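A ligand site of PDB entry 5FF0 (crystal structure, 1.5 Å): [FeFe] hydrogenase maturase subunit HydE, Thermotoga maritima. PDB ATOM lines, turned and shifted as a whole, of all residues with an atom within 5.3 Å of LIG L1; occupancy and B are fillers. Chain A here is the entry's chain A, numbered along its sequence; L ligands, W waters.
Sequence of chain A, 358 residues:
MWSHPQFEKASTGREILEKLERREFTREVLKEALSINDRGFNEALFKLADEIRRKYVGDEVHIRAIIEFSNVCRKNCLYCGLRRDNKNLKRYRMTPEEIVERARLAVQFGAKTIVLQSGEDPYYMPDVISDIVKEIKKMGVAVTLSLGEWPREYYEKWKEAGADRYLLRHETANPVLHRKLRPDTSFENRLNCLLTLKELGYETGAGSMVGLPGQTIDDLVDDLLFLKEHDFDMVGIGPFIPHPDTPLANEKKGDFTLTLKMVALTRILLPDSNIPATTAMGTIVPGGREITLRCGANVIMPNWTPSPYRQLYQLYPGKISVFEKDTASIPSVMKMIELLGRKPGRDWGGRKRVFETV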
ATOM      1  N   TYR A  79      15.855  -6.931  11.305  1.00  0.00           N
ATOM      2  CA  TYR A  79      15.579  -6.681   9.864  1.00  0.00           C
ATOM      3  C   TYR A  79      15.598  -5.201   9.493  1.00  0.00           C
ATOM      4  O   TYR A  79      15.691  -4.844   8.362  1.00  0.00           O
ATOM      5  CB  TYR A  79      14.236  -7.293   9.465  1.00  0.00           C
ATOM      6  CG  TYR A  79      13.101  -7.055  10.445  1.00  0.00           C
ATOM      7  CD1 TYR A  79      12.419  -5.820  10.472  1.00  0.00           C
ATOM      8  CD2 TYR A  79      12.703  -8.034  11.353  1.00  0.00           C
ATOM      9  CE1 TYR A  79      11.388  -5.594  11.378  1.00  0.00           C
ATOM     10  CE2 TYR A  79      11.687  -7.783  12.267  1.00  0.00           C
ATOM     11  CZ  TYR A  79      11.024  -6.576  12.255  1.00  0.00           C
ATOM     12  OH  TYR A  79      10.093  -6.407  13.170  1.00  0.00           O
ATOM     13  N   CYS A  80      15.408  -4.315  10.467  1.00  0.00           N
ATOM     14  CA  CYS A  80      15.103  -2.921  10.188  1.00  0.00           C
ATOM     15  C   CYS A  80      16.267  -1.950  10.102  1.00  0.00           C
ATOM     16  O   CYS A  80      17.043  -1.933  10.990  1.00  0.00           O
ATOM     17  CB  CYS A  80      14.185  -2.457  11.286  1.00  0.00           C
ATOM     18  SG  CYS A  80      13.509  -0.777  11.019  1.00  0.00           S
ATOM     19  N   GLY A  81      16.335  -1.086   9.092  1.00  0.00           N
ATOM     20  CA  GLY A  81      17.331  -0.078   8.992  1.00  0.00           C
ATOM     21  C   GLY A  81      17.351   1.003  10.029  1.00  0.00           C
ATOM     22  O   GLY A  81      18.343   1.736  10.148  1.00  0.00           O
ATOM     23  N   GLN A 117       3.721   7.865  11.284  1.00  0.00           N
ATOM     24  CA  GLN A 117       4.554   6.703  11.552  1.00  0.00           C
ATOM     25  C   GLN A 117       5.900   7.188  12.059  1.00  0.00           C
ATOM     26  O   GLN A 117       6.415   8.211  11.624  1.00  0.00           O
ATOM     27  CB  GLN A 117       4.759   5.842  10.324  1.00  0.00           C
ATOM     28  CG  GLN A 117       5.433   4.518  10.608  1.00  0.00           C
ATOM     29  CD  GLN A 117       5.599   3.593   9.414  1.00  0.00           C
ATOM     30  OE1 GLN A 117       6.544   3.726   8.695  1.00  0.00           O
ATOM     31  NE2 GLN A 117       4.737   2.715   9.229  1.00  0.00           N
ATOM     32  N   ARG A 169       1.828  -4.151  12.648  1.00  0.00           N
ATOM     33  CA  ARG A 169       1.955  -5.434  12.003  1.00  0.00           C
ATOM     34  C   ARG A 169       2.370  -6.435  13.020  1.00  0.00           C
ATOM     35  O   ARG A 169       3.184  -6.165  13.871  1.00  0.00           O
ATOM     36  CB  ARG A 169       2.990  -5.349  10.939  1.00  0.00           C
ATOM     37  CG  ARG A 169       2.465  -4.689   9.695  1.00  0.00           C
ATOM     38  CD  ARG A 169       3.514  -4.827   8.624  1.00  0.00           C
ATOM     39  NE  ARG A 169       3.223  -4.022   7.471  1.00  0.00           N
ATOM     40  CZ  ARG A 169       3.871  -4.127   6.333  1.00  0.00           C
ATOM     41  NH1 ARG A 169       4.865  -4.973   6.219  1.00  0.00           N
ATOM     42  NH2 ARG A 169       3.470  -3.370   5.312  1.00  0.00           N
ATOM     43  N   GLU A 171       4.118  -9.007  12.219  1.00  0.00           N
ATOM     44  CA  GLU A 171       5.441  -9.299  11.699  1.00  0.00           C
ATOM     45  C   GLU A 171       5.641 -10.787  11.325  1.00  0.00           C
ATOM     46  O   GLU A 171       5.938 -11.097  10.185  1.00  0.00           O
ATOM     47  CB  GLU A 171       6.582  -8.791  12.597  1.00  0.00           C
ATOM     48  CG  GLU A 171       6.447  -7.346  13.028  1.00  0.00           C
ATOM     49  CD  GLU A 171       6.408  -6.326  11.910  1.00  0.00           C
ATOM     50  OE1 GLU A 171       6.406  -6.686  10.731  1.00  0.00           O
ATOM     51  OE2 GLU A 171       6.418  -5.093  12.249  1.00  0.00           O
ATOM     52  N   ARG A 190       3.240  -8.277  21.318  1.00  0.00           N
ATOM     53  CA  ARG A 190       2.667  -7.703  20.089  1.00  0.00           C
ATOM     54  C   ARG A 190       1.195  -7.950  19.990  1.00  0.00           C
ATOM     55  O   ARG A 190       0.382  -7.058  19.697  1.00  0.00           O
ATOM     56  CB  ARG A 190       3.405  -8.327  18.879  1.00  0.00           C
ATOM     57  CG  ARG A 190       3.264  -7.555  17.556  1.00  0.00           C
ATOM     58  CD  ARG A 190       4.139  -6.316  17.612  1.00  0.00           C
ATOM     59  NE  ARG A 190       4.263  -5.674  16.291  1.00  0.00           N
ATOM     60  CZ  ARG A 190       4.922  -4.535  16.098  1.00  0.00           C
ATOM     61  NH1 ARG A 190       5.531  -3.920  17.097  1.00  0.00           N
ATOM     62  NH2 ARG A 190       4.913  -3.989  14.898  1.00  0.00           N
ATOM     63  N   SER A 208       2.263  -8.842   8.090  1.00  0.00           N
ATOM     64  CA  SER A 208       3.500  -9.575   8.238  1.00  0.00           C
ATOM     65  C   SER A 208       4.392  -9.393   7.114  1.00  0.00           C
ATOM     66  O   SER A 208       3.998  -8.889   6.029  1.00  0.00           O
ATOM     67  CB  SER A 208       3.199 -11.053   8.484  1.00  0.00           C
ATOM     68  OG  SER A 208       2.329 -11.553   7.481  1.00  0.00           O
ATOM     69  N   MET A 209       5.659  -9.766   7.301  1.00  0.00           N
ATOM     70  CA  MET A 209       6.637  -9.813   6.189  1.00  0.00           C
ATOM     71  C   MET A 209       6.700 -11.256   5.668  1.00  0.00           C
ATOM     72  O   MET A 209       6.439 -12.211   6.394  1.00  0.00           O
ATOM     73  CB  MET A 209       8.002  -9.372   6.609  1.00  0.00           C
ATOM     74  CG  MET A 209       8.077  -7.805   6.839  1.00  0.00           C
ATOM     75  SD  MET A 209       9.660  -7.289   7.546  1.00  0.00           S
ATOM     76  CE  MET A 209       9.389  -7.801   9.205  1.00  0.00           C
ATOM     77  N   PRO A 239       7.168  -7.986   1.218  1.00  0.00           N
ATOM     78  CA  PRO A 239       8.341  -8.862   1.276  1.00  0.00           C
ATOM     79  C   PRO A 239       9.379  -8.306   2.188  1.00  0.00           C
ATOM     80  O   PRO A 239       9.560  -7.125   2.314  1.00  0.00           O
ATOM     81  CB  PRO A 239       8.865  -8.828  -0.169  1.00  0.00           C
ATOM     82  CG  PRO A 239       8.530  -7.431  -0.599  1.00  0.00           C
ATOM     83  CD  PRO A 239       7.186  -7.176   0.011  1.00  0.00           C
ATOM     84  N   PHE A 240      10.149  -9.213   2.840  1.00  0.00           N
ATOM     85  CA  PHE A 240      11.369  -8.813   3.509  1.00  0.00           C
ATOM     86  C   PHE A 240      12.403  -8.358   2.527  1.00  0.00           C
ATOM     87  O   PHE A 240      12.631  -9.042   1.510  1.00  0.00           O
ATOM     88  CB  PHE A 240      11.928 -10.003   4.292  1.00  0.00           C
ATOM     89  CG  PHE A 240      13.324  -9.806   4.737  1.00  0.00           C
ATOM     90  CD1 PHE A 240      13.678  -8.849   5.676  1.00  0.00           C
ATOM     91  CD2 PHE A 240      14.294 -10.655   4.222  1.00  0.00           C
ATOM     92  CE1 PHE A 240      15.014  -8.662   6.016  1.00  0.00           C
ATOM     93  CE2 PHE A 240      15.640 -10.497   4.640  1.00  0.00           C
ATOM     94  CZ  PHE A 240      15.989  -9.496   5.509  1.00  0.00           C
ATOM     95  N   ILE A 241      13.020  -7.199   2.755  1.00  0.00           N
ATOM     96  CA  ILE A 241      14.029  -6.653   1.877  1.00  0.00           C
ATOM     97  C   ILE A 241      15.281  -6.409   2.760  1.00  0.00           C
ATOM     98  O   ILE A 241      15.279  -5.542   3.647  1.00  0.00           O
ATOM     99  CB  ILE A 241      13.584  -5.394   1.162  1.00  0.00           C
ATOM    100  CG1 ILE A 241      12.341  -5.639   0.319  1.00  0.00           C
ATOM    101  CG2 ILE A 241      14.735  -4.788   0.368  1.00  0.00           C
ATOM    102  CD1 ILE A 241      11.717  -4.364  -0.267  1.00  0.00           C
ATOM    103  N   PRO A 242      16.400  -7.141   2.534  1.00  0.00           N
ATOM    104  CA  PRO A 242      17.550  -6.965   3.418  1.00  0.00           C
ATOM    105  C   PRO A 242      18.141  -5.585   3.340  1.00  0.00           C
ATOM    106  O   PRO A 242      18.280  -4.970   2.283  1.00  0.00           O
ATOM    107  CB  PRO A 242      18.536  -8.029   2.909  1.00  0.00           C
ATOM    108  CG  PRO A 242      18.156  -8.222   1.497  1.00  0.00           C
ATOM    109  CD  PRO A 242      16.688  -8.014   1.384  1.00  0.00           C
ATOM    110  N   HIS A 243      18.537  -5.098   4.511  1.00  0.00           N
ATOM    111  CA  HIS A 243      19.120  -3.788   4.635  1.00  0.00           C
ATOM    112  C   HIS A 243      20.617  -3.978   5.017  1.00  0.00           C
ATOM    113  O   HIS A 243      20.972  -4.717   5.925  1.00  0.00           O
ATOM    114  CB  HIS A 243      18.396  -2.971   5.715  1.00  0.00           C
ATOM    115  CG  HIS A 243      18.805  -1.543   5.799  1.00  0.00           C
ATOM    116  ND1 HIS A 243      20.071  -1.125   6.154  1.00  0.00           N
ATOM    117  CD2 HIS A 243      18.093  -0.432   5.580  1.00  0.00           C
ATOM    118  CE1 HIS A 243      20.112   0.188   6.119  1.00  0.00           C
ATOM    119  NE2 HIS A 243      18.924   0.633   5.786  1.00  0.00           N
ATOM    120  N   THR A 278       1.603  -2.251  -0.762  1.00  0.00           N
ATOM    121  CA  THR A 278       2.642  -1.590   0.004  1.00  0.00           C
ATOM    122  C   THR A 278       3.819  -1.102  -0.856  1.00  0.00           C
ATOM    123  O   THR A 278       4.096  -1.596  -1.894  1.00  0.00           O
ATOM    124  CB  THR A 278       3.179  -2.521   1.096  1.00  0.00           C
ATOM    125  OG1 THR A 278       3.751  -3.697   0.532  1.00  0.00           O
ATOM    126  CG2 THR A 278       2.097  -2.894   2.094  1.00  0.00           C
ATOM    127  N   THR A 279       4.521  -0.091  -0.315  1.00  0.00           N
ATOM    128  CA  THR A 279       5.658   0.446  -0.988  1.00  0.00           C
ATOM    129  C   THR A 279       6.753  -0.618  -1.164  1.00  0.00           C
ATOM    130  O   THR A 279       7.422  -0.632  -2.159  1.00  0.00           O
ATOM    131  CB  THR A 279       6.206   1.672  -0.274  1.00  0.00           C
ATOM    132  OG1 THR A 279       5.266   2.715  -0.366  1.00  0.00           O
ATOM    133  CG2 THR A 279       7.503   2.166  -0.887  1.00  0.00           C
ATOM    134  N   ALA A 280       6.867  -1.548  -0.224  1.00  0.00           N
ATOM    135  CA  ALA A 280       7.831  -2.660  -0.378  1.00  0.00           C
ATOM    136  C   ALA A 280       7.564  -3.508  -1.638  1.00  0.00           C
ATOM    137  O   ALA A 280       8.478  -3.875  -2.330  1.00  0.00           O
ATOM    138  CB  ALA A 280       7.880  -3.544   0.854  1.00  0.00           C
ATOM    139  N   MET A 281       6.284  -3.716  -1.947  1.00  0.00           N
ATOM    140  CA  MET A 281       5.928  -4.450  -3.176  1.00  0.00           C
ATOM    141  C   MET A 281       6.408  -3.697  -4.430  1.00  0.00           C
ATOM    142  O   MET A 281       6.798  -4.269  -5.387  1.00  0.00           O
ATOM    143  CB  MET A 281       4.397  -4.679  -3.231  1.00  0.00           C
ATOM    144  CG  MET A 281       3.916  -5.752  -2.239  1.00  0.00           C
ATOM    145  SD  MET A 281       4.626  -7.344  -2.596  1.00  0.00           S
ATOM    146  CE  MET A 281       3.222  -8.147  -3.427  1.00  0.00           C
ATOM    147  N   LEU A 315      13.660   1.813   6.078  1.00  0.00           N
ATOM    148  CA  LEU A 315      13.572   0.555   6.795  1.00  0.00           C
ATOM    149  C   LEU A 315      14.287  -0.514   5.972  1.00  0.00           C
ATOM    150  O   LEU A 315      14.848  -1.403   6.499  1.00  0.00           O
ATOM    151  CB  LEU A 315      12.109   0.143   6.945  1.00  0.00           C
ATOM    152  CG  LEU A 315      11.147   1.193   7.440  1.00  0.00           C
ATOM    153  CD1 LEU A 315       9.718   0.632   7.555  1.00  0.00           C
ATOM    154  CD2 LEU A 315      11.569   1.729   8.686  1.00  0.00           C
ATOM    155  N   TYR A 316      14.194  -0.367   4.660  1.00  0.00           N
ATOM    156  CA  TYR A 316      14.814  -1.208   3.697  1.00  0.00           C
ATOM    157  C   TYR A 316      15.328  -0.297   2.605  1.00  0.00           C
ATOM    158  O   TYR A 316      14.825   0.795   2.390  1.00  0.00           O
ATOM    159  CB  TYR A 316      13.846  -2.229   3.098  1.00  0.00           C
ATOM    160  CG  TYR A 316      12.541  -1.657   2.626  1.00  0.00           C
ATOM    161  CD1 TYR A 316      12.422  -1.142   1.361  1.00  0.00           C
ATOM    162  CD2 TYR A 316      11.461  -1.623   3.466  1.00  0.00           C
ATOM    163  CE1 TYR A 316      11.269  -0.612   0.927  1.00  0.00           C
ATOM    164  CE2 TYR A 316      10.275  -1.037   3.050  1.00  0.00           C
ATOM    165  CZ  TYR A 316      10.192  -0.552   1.793  1.00  0.00           C
ATOM    166  OH  TYR A 316       9.079   0.021   1.327  1.00  0.00           O
HETATM  167  N1  LIG L   1      11.963  -5.112   4.688  1.00  0.00           N
HETATM  168  C1  LIG L   1      11.665  -4.102   6.713  1.00  0.00           C
HETATM  169  C2  LIG L   1      10.626  -3.222   8.383  1.00  0.00           C
HETATM  170  C3  LIG L   1      10.647  -5.037   4.457  1.00  0.00           C
HETATM  171  C4  LIG L   1      12.479  -4.637   5.831  1.00  0.00           C
HETATM  172  N2  LIG L   1       9.860  -4.490   5.352  1.00  0.00           N
HETATM  173  C5  LIG L   1      10.342  -4.049   6.463  1.00  0.00           C
HETATM  174  O1  LIG L   1       7.304   0.678   3.091  1.00  0.00           O
HETATM  175  C6  LIG L   1       6.321  -0.073   3.208  1.00  0.00           C
HETATM  176  O2  LIG L   1       6.103  -1.061   2.605  1.00  0.00           O
HETATM  177  C7  LIG L   1       5.484   0.197   4.439  1.00  0.00           C
HETATM  178  N3  LIG L   1       4.129  -0.284   4.137  1.00  0.00           N
HETATM  179  C8  LIG L   1       6.141  -0.395   5.676  1.00  0.00           C
HETATM  180  S1  LIG L   1       5.084  -0.130   7.203  1.00  0.00           S
HETATM  181  C9  LIG L   1       6.190  -0.838   8.629  1.00  0.00           C
HETATM  182  C10 LIG L   1       6.560  -2.244   8.453  1.00  0.00           C
HETATM  183  O3  LIG L   1       7.679  -2.266   7.590  1.00  0.00           O
HETATM  184  C11 LIG L   1       7.104  -2.893   9.703  1.00  0.00           C
HETATM  185  O4  LIG L   1       5.988  -3.267  10.522  1.00  0.00           O
HETATM  186  C12 LIG L   1       7.778  -4.095   9.000  1.00  0.00           C
HETATM  187  O5  LIG L   1       6.842  -5.161   8.663  1.00  0.00           O
HETATM  188  C13 LIG L   1       8.253  -3.504   7.630  1.00  0.00           C
HETATM  189  N4  LIG L   1       9.679  -3.552   7.471  1.00  0.00           N
HETATM  190  N5  LIG L   1      11.824  -3.548   7.909  1.00  0.00           N
HETATM  191  N6  LIG L   1      13.774  -4.693   5.982  1.00  0.00           N
HETATM  192  N1  LG2 L   2       7.995   1.150  14.613  1.00  0.00           N
HETATM  193  C1  LG2 L   2       6.566   0.844  14.291  1.00  0.00           C
HETATM  194  C2  LG2 L   2       6.454  -0.654  14.326  1.00  0.00           C
HETATM  195  O1  LG2 L   2       5.345  -1.134  14.319  1.00  0.00           O
HETATM  196  C3  LG2 L   2       6.192   1.424  12.901  1.00  0.00           C
HETATM  197  C4  LG2 L   2       6.599   0.528  11.745  1.00  0.00           C
HETATM  198  S1  LG2 L   2       8.397   0.304  11.516  1.00  0.00           S
HETATM  199  C5  LG2 L   2       8.670   1.993  11.092  1.00  0.00           C
HETATM  200  O2  LG2 L   2       7.510  -1.384  14.276  1.00  0.00           O
HETATM  201 SE1  LG3 L   3      13.751  -1.236  14.803  1.00  0.00          SE
HETATM  202 FE1  LG3 L   3      12.301  -0.654  12.964  1.00  0.00          FE
HETATM  203 FE2  LG3 L   3      11.627  -2.363  14.954  1.00  0.00          FE
HETATM  204 FE3  LG3 L   3      12.109   0.295  15.463  1.00  0.00          FE
HETATM  205 SE2  LG3 L   3      11.346   1.365  13.492  1.00  0.00          SE
HETATM  206 FE4  LG3 L   3       9.616  -0.326  13.937  1.00  0.00          FE
HETATM  207 SE3  LG3 L   3      10.565  -2.340  12.788  1.00  0.00          SE
HETATM  208 SE4  LG3 L   3      10.272  -1.022  16.312  1.00  0.00          SE
HETATM  209  O   HOH W   1       3.148   1.351   1.955  1.00  0.00           O
HETATM  210  O   HOH W   2       2.350   2.242   5.637  1.00  0.00           O
HETATM  211  O   HOH W   3       5.474  -3.622   3.227  1.00  0.00           O
HETATM  212  O   HOH W   4       3.974  -2.137  11.949  1.00  0.00           O
HETATM  213  O   HOH W   5       8.600   2.261   4.714  1.00  0.00           O
HETATM  214  O   HOH W   6       7.392  -5.293   4.055  1.00  0.00           O
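Pro 239 touches LIG L1 (O to C3, 3.2 Å).
Phe 240 touches LIG L1 (C to N1, 3.9 Å).
Thr 278 touches LIG L1 (CB to O2, 3.6 Å).
Hydrophobic or aromatic side chains that line LIG L1: Tyr 79, Met 209, Ile 241, Ala 280, Leu 315 and Tyr 316.
FE4 of LG3 L3 is bound by N1 of LG2 L2, 2.3 Å away.
OE2 of Glu 171 is in hydrogen-bond range of O4 of LIG L1 (2.5 Å).
The side-chain hydroxyl (OH) of Tyr 316 sits at hydrogen-bond distance from an oxygen (O1) of LIG L1, at 2.6 Å.
N of Ile 241 is in hydrogen-bond range of N1 of LIG L1.
O of Ile 241 is in hydrogen-bond range of N6 of LIG L1, 2.9 Å away.
The backbone NH (N) of Ala 280 lies within hydrogen-bond range of an oxygen (O2) of LIG L1 (3.0 Å).
O of Tyr 79 lies within hydrogen-bond range of N6 of LIG L1 (3.1 Å).
An oxygen (O5) of LIG L1 is in hydrogen-bond range of the guanidinium group of Arg 169, 3.1 Å away.
The side-chain sulfur (SD) of Met 209 sits close to an oxygen (O5) of LIG L1, at 3.7 Å.
The backbone NH (N) of Thr 279 sits at hydrogen-bond distance from an oxygen (O2) of LIG L1 (3.5 Å).
The backbone carbonyl oxygen (O) of Leu 315 lies within hydrogen-bond range of a nitrogen (N6) of LIG L1, at 3.5 Å.
S1 of LIG L1 lies close to NE2 of Gln 117 (3.5 Å).
NH2 of Arg 190 is in salt-bridge range of O1 of LG2 L2.
SG of Cys 80 binds FE1 of LG3 L3.
O of Glu 171 lies within hydrogen-bond range of N of Met 209, 3.2 Å away.
The guanidinium group of Arg 190 lies within salt-bridge range of the side-chain carboxylate of Glu 171.
The backbone NH of Ala 280 sits at hydrogen-bond distance from the side-chain hydroxyl of Tyr 316 (3.1 Å).
The backbone carbonyl oxygen (O) of Arg 169 lies within hydrogen-bond range of the guanidinium group (NE) of Arg 190 (2.7 Å).
O of Leu 315 lies within hydrogen-bond range of N of Gly 81.
Water W3 lies within hydrogen-bond range of an oxygen (O2) of LIG L1 (2.7 Å), the guanidinium group of Arg 169 (2.9 Å) and the side-chain hydroxyl of Thr 278 (3.2 Å).
Water W4 lies within hydrogen-bond range of O4 of LIG L1 (2.7 Å), O1 of LG2 L2 (2.9 Å) and N of Arg 169 (3.0 Å).
Water W1 bridges N3 of LIG L1 and N of Thr 279.
Water W6 lies within hydrogen-bond range of N2 of LIG L1 (2.9 Å), O of Pro 239 (3.3 Å) and NH1 of Arg 169 (3.3 Å).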
